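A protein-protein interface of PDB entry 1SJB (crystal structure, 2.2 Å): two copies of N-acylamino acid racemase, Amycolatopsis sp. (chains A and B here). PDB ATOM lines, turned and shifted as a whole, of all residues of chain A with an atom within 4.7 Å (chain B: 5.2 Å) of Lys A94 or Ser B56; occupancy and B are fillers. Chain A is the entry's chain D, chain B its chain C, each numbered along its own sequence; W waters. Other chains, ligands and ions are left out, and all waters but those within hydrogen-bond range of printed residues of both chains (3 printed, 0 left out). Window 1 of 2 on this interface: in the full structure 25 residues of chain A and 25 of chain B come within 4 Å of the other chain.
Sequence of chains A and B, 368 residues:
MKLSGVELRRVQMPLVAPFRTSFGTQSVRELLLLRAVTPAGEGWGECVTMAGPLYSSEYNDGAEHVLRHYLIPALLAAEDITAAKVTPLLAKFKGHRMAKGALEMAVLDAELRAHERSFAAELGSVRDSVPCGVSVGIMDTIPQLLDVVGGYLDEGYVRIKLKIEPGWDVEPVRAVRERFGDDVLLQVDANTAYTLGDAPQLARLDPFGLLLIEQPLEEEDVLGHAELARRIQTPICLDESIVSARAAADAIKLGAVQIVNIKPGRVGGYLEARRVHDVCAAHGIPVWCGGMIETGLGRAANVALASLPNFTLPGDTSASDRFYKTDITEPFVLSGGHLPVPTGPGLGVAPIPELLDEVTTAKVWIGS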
ATOM      1  N   ALA A  91      -1.170 -20.036 -11.878  1.00  0.00           N
ATOM      2  CA  ALA A  91      -0.294 -19.493 -10.894  1.00  0.00           C
ATOM      3  C   ALA A  91      -0.114 -17.977 -11.023  1.00  0.00           C
ATOM      4  O   ALA A  91      -0.131 -17.258 -10.022  1.00  0.00           O
ATOM      5  CB  ALA A  91       1.018 -20.282 -10.889  1.00  0.00           C
ATOM      6  N   LYS A  92       0.051 -17.467 -12.253  1.00  0.00           N
ATOM      7  CA  LYS A  92       0.257 -16.024 -12.428  1.00  0.00           C
ATOM      8  C   LYS A  92      -0.803 -15.168 -11.719  1.00  0.00           C
ATOM      9  O   LYS A  92      -0.620 -13.983 -11.472  1.00  0.00           O
ATOM     10  CB  LYS A  92       0.345 -15.637 -13.883  1.00  0.00           C
ATOM     11  CG  LYS A  92      -1.011 -15.757 -14.543  1.00  0.00           C
ATOM     12  CD  LYS A  92      -1.107 -14.935 -15.803  1.00  0.00           C
ATOM     13  CE  LYS A  92      -0.599 -15.696 -17.024  1.00  0.00           C
ATOM     14  NZ  LYS A  92      -1.556 -16.689 -17.576  1.00  0.00           N
ATOM     15  N   PHE A  93      -1.934 -15.775 -11.383  1.00  0.00           N
ATOM     16  CA  PHE A  93      -2.964 -15.021 -10.726  1.00  0.00           C
ATOM     17  C   PHE A  93      -2.879 -15.230  -9.253  1.00  0.00           C
ATOM     18  O   PHE A  93      -2.987 -16.360  -8.785  1.00  0.00           O
ATOM     19  CB  PHE A  93      -4.379 -15.353 -11.230  1.00  0.00           C
ATOM     20  CG  PHE A  93      -4.446 -15.331 -12.730  1.00  0.00           C
ATOM     21  CD1 PHE A  93      -4.676 -16.524 -13.415  1.00  0.00           C
ATOM     22  CD2 PHE A  93      -4.252 -14.145 -13.449  1.00  0.00           C
ATOM     23  CE1 PHE A  93      -4.718 -16.543 -14.809  1.00  0.00           C
ATOM     24  CE2 PHE A  93      -4.308 -14.142 -14.843  1.00  0.00           C
ATOM     25  CZ  PHE A  93      -4.555 -15.345 -15.512  1.00  0.00           C
ATOM     26  N   LYS A  94      -2.704 -14.124  -8.542  1.00  0.00           N
ATOM     27  CA  LYS A  94      -2.577 -14.120  -7.105  1.00  0.00           C
ATOM     28  C   LYS A  94      -3.891 -14.353  -6.358  1.00  0.00           C
ATOM     29  O   LYS A  94      -4.897 -13.681  -6.611  1.00  0.00           O
ATOM     30  CB  LYS A  94      -1.797 -12.884  -6.615  1.00  0.00           C
ATOM     31  CG  LYS A  94      -0.486 -12.705  -7.373  1.00  0.00           C
ATOM     32  CD  LYS A  94       0.672 -13.286  -6.633  1.00  0.00           C
ATOM     33  CE  LYS A  94       1.982 -13.165  -7.373  1.00  0.00           C
ATOM     34  NZ  LYS A  94       3.155 -13.408  -6.515  1.00  0.00           N
ATOM     35  N   GLY A  95      -3.874 -15.336  -5.438  1.00  0.00           N
ATOM     36  CA  GLY A  95      -5.028 -15.672  -4.581  1.00  0.00           C
ATOM     37  C   GLY A  95      -6.175 -16.417  -5.284  1.00  0.00           C
ATOM     38  O   GLY A  95      -5.953 -17.306  -6.126  1.00  0.00           O
ATOM     39  N   HIS A  96      -7.420 -16.053  -4.899  1.00  0.00           N
ATOM     40  CA  HIS A  96      -8.667 -16.620  -5.475  1.00  0.00           C
ATOM     41  C   HIS A  96      -8.719 -18.139  -5.335  1.00  0.00           C
ATOM     42  O   HIS A  96      -9.183 -18.881  -6.199  1.00  0.00           O
ATOM     43  CB  HIS A  96      -8.830 -16.173  -6.964  1.00  0.00           C
ATOM     44  CG  HIS A  96      -9.030 -14.700  -7.001  1.00  0.00           C
ATOM     45  ND1 HIS A  96     -10.266 -14.162  -6.656  1.00  0.00           N
ATOM     46  CD2 HIS A  96      -8.149 -13.673  -7.224  1.00  0.00           C
ATOM     47  CE1 HIS A  96     -10.121 -12.828  -6.686  1.00  0.00           C
ATOM     48  NE2 HIS A  96      -8.860 -12.491  -7.013  1.00  0.00           N
ATOM     49  N   GLY B  52      -5.151  -6.571 -13.779  1.00  0.00           N
ATOM     50  CA  GLY B  52      -5.231  -7.973 -13.354  1.00  0.00           C
ATOM     51  C   GLY B  52      -4.599  -8.202 -11.999  1.00  0.00           C
ATOM     52  O   GLY B  52      -3.998  -7.328 -11.390  1.00  0.00           O
ATOM     53  N   PRO B  53      -4.809  -9.392 -11.509  1.00  0.00           N
ATOM     54  CA  PRO B  53      -4.335  -9.771 -10.195  1.00  0.00           C
ATOM     55  C   PRO B  53      -2.950 -10.426 -10.200  1.00  0.00           C
ATOM     56  O   PRO B  53      -2.805 -11.561  -9.761  1.00  0.00           O
ATOM     57  CB  PRO B  53      -5.398 -10.739  -9.670  1.00  0.00           C
ATOM     58  CG  PRO B  53      -6.223 -11.206 -10.876  1.00  0.00           C
ATOM     59  CD  PRO B  53      -5.842 -10.295 -12.043  1.00  0.00           C
ATOM     60  N   LEU B  54      -1.946  -9.667 -10.657  1.00  0.00           N
ATOM     61  CA  LEU B  54      -0.581 -10.144 -10.772  1.00  0.00           C
ATOM     62  C   LEU B  54       0.383  -9.823  -9.642  1.00  0.00           C
ATOM     63  O   LEU B  54       1.271 -10.618  -9.387  1.00  0.00           O
ATOM     64  CB  LEU B  54       0.002  -9.708 -12.112  1.00  0.00           C
ATOM     65  CG  LEU B  54      -1.053  -9.849 -13.198  1.00  0.00           C
ATOM     66  CD1 LEU B  54      -0.448  -9.409 -14.512  1.00  0.00           C
ATOM     67  CD2 LEU B  54      -1.478 -11.314 -13.308  1.00  0.00           C
ATOM     68  N   TYR B  55       0.251  -8.655  -9.000  1.00  0.00           N
ATOM     69  CA  TYR B  55       1.141  -8.303  -7.861  1.00  0.00           C
ATOM     70  C   TYR B  55       0.539  -8.958  -6.624  1.00  0.00           C
ATOM     71  O   TYR B  55       1.210  -9.585  -5.811  1.00  0.00           O
ATOM     72  CB  TYR B  55       1.251  -6.763  -7.670  1.00  0.00           C
ATOM     73  CG  TYR B  55       1.821  -6.199  -6.344  1.00  0.00           C
ATOM     74  CD1 TYR B  55       1.044  -6.020  -5.193  1.00  0.00           C
ATOM     75  CD2 TYR B  55       3.139  -5.734  -6.298  1.00  0.00           C
ATOM     76  CE1 TYR B  55       1.580  -5.451  -4.030  1.00  0.00           C
ATOM     77  CE2 TYR B  55       3.698  -5.174  -5.147  1.00  0.00           C
ATOM     78  CZ  TYR B  55       2.912  -5.028  -4.001  1.00  0.00           C
ATOM     79  OH  TYR B  55       3.441  -4.488  -2.837  1.00  0.00           O
ATOM     80  N   SER B  56      -0.789  -8.808  -6.548  1.00  0.00           N
ATOM     81  CA  SER B  56      -1.598  -9.336  -5.488  1.00  0.00           C
ATOM     82  C   SER B  56      -2.936  -9.729  -6.037  1.00  0.00           C
ATOM     83  O   SER B  56      -3.230  -9.537  -7.199  1.00  0.00           O
ATOM     84  CB  SER B  56      -1.773  -8.366  -4.333  1.00  0.00           C
ATOM     85  OG  SER B  56      -2.679  -7.332  -4.701  1.00  0.00           O
ATOM     86  N   SER B  57      -3.763 -10.244  -5.171  1.00  0.00           N
ATOM     87  CA  SER B  57      -5.069 -10.703  -5.548  1.00  0.00           C
ATOM     88  C   SER B  57      -6.037  -9.608  -6.012  1.00  0.00           C
ATOM     89  O   SER B  57      -7.053  -9.870  -6.658  1.00  0.00           O
ATOM     90  CB  SER B  57      -5.667 -11.414  -4.335  1.00  0.00           C
ATOM     91  OG  SER B  57      -5.778 -10.519  -3.229  1.00  0.00           O
ATOM     92  N   GLU B  58      -5.771  -8.393  -5.620  1.00  0.00           N
ATOM     93  CA  GLU B  58      -6.646  -7.309  -5.964  1.00  0.00           C
ATOM     94  C   GLU B  58      -6.370  -6.783  -7.356  1.00  0.00           C
ATOM     95  O   GLU B  58      -5.213  -6.612  -7.763  1.00  0.00           O
ATOM     96  CB  GLU B  58      -6.585  -6.157  -4.922  1.00  0.00           C
ATOM     97  CG  GLU B  58      -7.135  -6.519  -3.507  1.00  0.00           C
ATOM     98  CD  GLU B  58      -6.826  -5.507  -2.404  1.00  0.00           C
ATOM     99  OE1 GLU B  58      -5.859  -5.595  -1.669  1.00  0.00           O
ATOM    100  OE2 GLU B  58      -7.725  -4.568  -2.269  1.00  0.00           O
ATOM    101  N   MET B  98      -6.300  -2.502  -0.624  1.00  0.00           N
ATOM    102  CA  MET B  98      -6.053  -1.399  -1.525  1.00  0.00           C
ATOM    103  C   MET B  98      -7.323  -0.613  -1.763  1.00  0.00           C
ATOM    104  O   MET B  98      -7.295   0.606  -1.820  1.00  0.00           O
ATOM    105  CB  MET B  98      -5.390  -1.837  -2.823  1.00  0.00           C
ATOM    106  CG  MET B  98      -4.036  -2.397  -2.529  1.00  0.00           C
ATOM    107  SD  MET B  98      -3.334  -3.156  -3.992  1.00  0.00           S
ATOM    108  CE  MET B  98      -4.765  -4.156  -4.402  1.00  0.00           C
ATOM    109  N   ASN B 191       9.732  -9.020  -6.967  1.00  0.00           N
ATOM    110  CA  ASN B 191       8.302  -9.166  -6.927  1.00  0.00           C
ATOM    111  C   ASN B 191       7.884 -10.616  -6.850  1.00  0.00           C
ATOM    112  O   ASN B 191       7.049 -11.046  -7.668  1.00  0.00           O
ATOM    113  CB  ASN B 191       7.518  -8.384  -8.022  1.00  0.00           C
ATOM    114  CG  ASN B 191       7.644  -6.871  -7.896  1.00  0.00           C
ATOM    115  OD1 ASN B 191       8.390  -6.245  -8.633  1.00  0.00           O
ATOM    116  ND2 ASN B 191       6.912  -6.272  -6.944  1.00  0.00           N
ATOM    117  N   THR B 192       8.446 -11.341  -5.848  1.00  0.00           N
ATOM    118  CA  THR B 192       8.150 -12.774  -5.579  1.00  0.00           C
ATOM    119  C   THR B 192       8.629 -13.794  -6.622  1.00  0.00           C
ATOM    120  O   THR B 192       8.134 -14.916  -6.661  1.00  0.00           O
ATOM    121  CB  THR B 192       6.649 -13.004  -5.341  1.00  0.00           C
ATOM    122  OG1 THR B 192       5.957 -13.297  -6.544  1.00  0.00           O
ATOM    123  CG2 THR B 192       6.039 -11.797  -4.666  1.00  0.00           C
ATOM    124  N   GLU B 219       4.650 -13.722  -1.147  1.00  0.00           N
ATOM    125  CA  GLU B 219       4.022 -12.919  -0.125  1.00  0.00           C
ATOM    126  C   GLU B 219       3.856 -13.661   1.182  1.00  0.00           C
ATOM    127  O   GLU B 219       4.133 -13.136   2.238  1.00  0.00           O
ATOM    128  CB  GLU B 219       2.631 -12.483  -0.651  1.00  0.00           C
ATOM    129  CG  GLU B 219       1.792 -11.591   0.297  1.00  0.00           C
ATOM    130  CD  GLU B 219       0.415 -11.191  -0.261  1.00  0.00           C
ATOM    131  OE1 GLU B 219       0.262 -10.680  -1.374  1.00  0.00           O
ATOM    132  OE2 GLU B 219      -0.595 -11.425   0.561  1.00  0.00           O
HETATM  133  O   HOH W   1       1.990 -12.816 -11.239  1.00  0.00           O
HETATM  134  O   HOH W   2       4.002 -11.101  -8.561  1.00  0.00           O
HETATM  135  O   HOH W   3       2.272 -14.356  -3.502  1.00  0.00           O
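Water W1 bridges the backbone carbonyl oxygen (O) of Lys A92 (2.9 Å) and the backbone carbonyl oxygen (O) of Leu B54 (3.0 Å).
Water W2 lies within hydrogen-bond range of the backbone carbonyl oxygen of Leu B54, the backbone carbonyl oxygen of Asn B191 and the side-chain amino group of Lys A94.
Water W3 lies within hydrogen-bond range of the side-chain amino group (NZ) of Lys A94 and the backbone NH (N) of Glu B219.
Printed residues of chain B within 4 Å of Lys A92: Pro B53 (3.7 Å) and Leu B54 (3.4 Å).
Printed residues of chain B within 4 Å of Phe A93: Pro B53 and Leu B54.
Lys A94 touches just these residues of chain B: Pro B53 (2.8 Å), Leu B54 (3.3 Å), Tyr B55 (3.8 Å), Ser B56 (3.4 Å), Ser B57 (3.2 Å) and Thr B192 (2.8 Å).
Gly B52 touches none of the printed residues of chain A.
Printed residues of chain A within 4 Å of Leu B54: Lys A92 (3.4 Å), Phe A93 (3.97 Å) and Lys A94 (3.3 Å).
Printed residues of chain A within 4 Å of Tyr B55: Lys A94.
Ser B56 touches just one residue of chain A: Lys A94.
Glu B58 touches none of the printed residues of chain A.
Printed residues of chain A within 4 Å of Thr B192: Lys A94.
The nearest printed residue of chain A that does not touch Ser B56 is Gly A95 (5.7 Å).
The nearest printed residue of chain B that does not touch Lys A92 is Tyr B55 (5.9 Å).
Of the 11 printed residues of chain B, 6 touch a printed residue of chain A.
Of the 6 printed residues of chain A, 4 touch a printed residue of chain B.
Hydrophobic or aromatic side chains of chain A that line the printed part of chain B: Phe A93 and His A96.
Among the printed residues, no Asp or Glu carboxylate lies within 4 Å of a Lys or Arg side-chain nitrogen of the other chain.
No position is printed for both chains.
Of the 11 pairs that touch across the chains among the printed residues, none has its exchanged pair printed and touching as well.
The side-chain hydroxyl (OG) of Ser B56 sits close to the backbone NH (N) of Glu B58 (3.4 Å).
O of Pro B53 sits at hydrogen-bond distance from N of Lys A94 (2.8 Å).
A ring nitrogen (NE2) of His A96 lies within hydrogen-bond range of the backbone carbonyl oxygen of Ser B57, at 3.2 Å.
OG1 of Thr B192 sits at hydrogen-bond distance from NZ of Lys A94, at 2.8 Å.
Among the printed residues, pairs that only touch across the chains: Lys A94 with Ser B57 (3.2 Å), Lys A94 with Leu B54 (3.3 Å), Lys A92 with Leu B54 (3.4 Å), Lys A94 with Ser B56 (3.4 Å), Phe A93 with Pro B53 (3.6 Å), Lys A92 with Pro B53 (3.7 Å), Lys A94 with Tyr B55 (3.8 Å) and Phe A93 with Leu B54 (3.97 Å).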
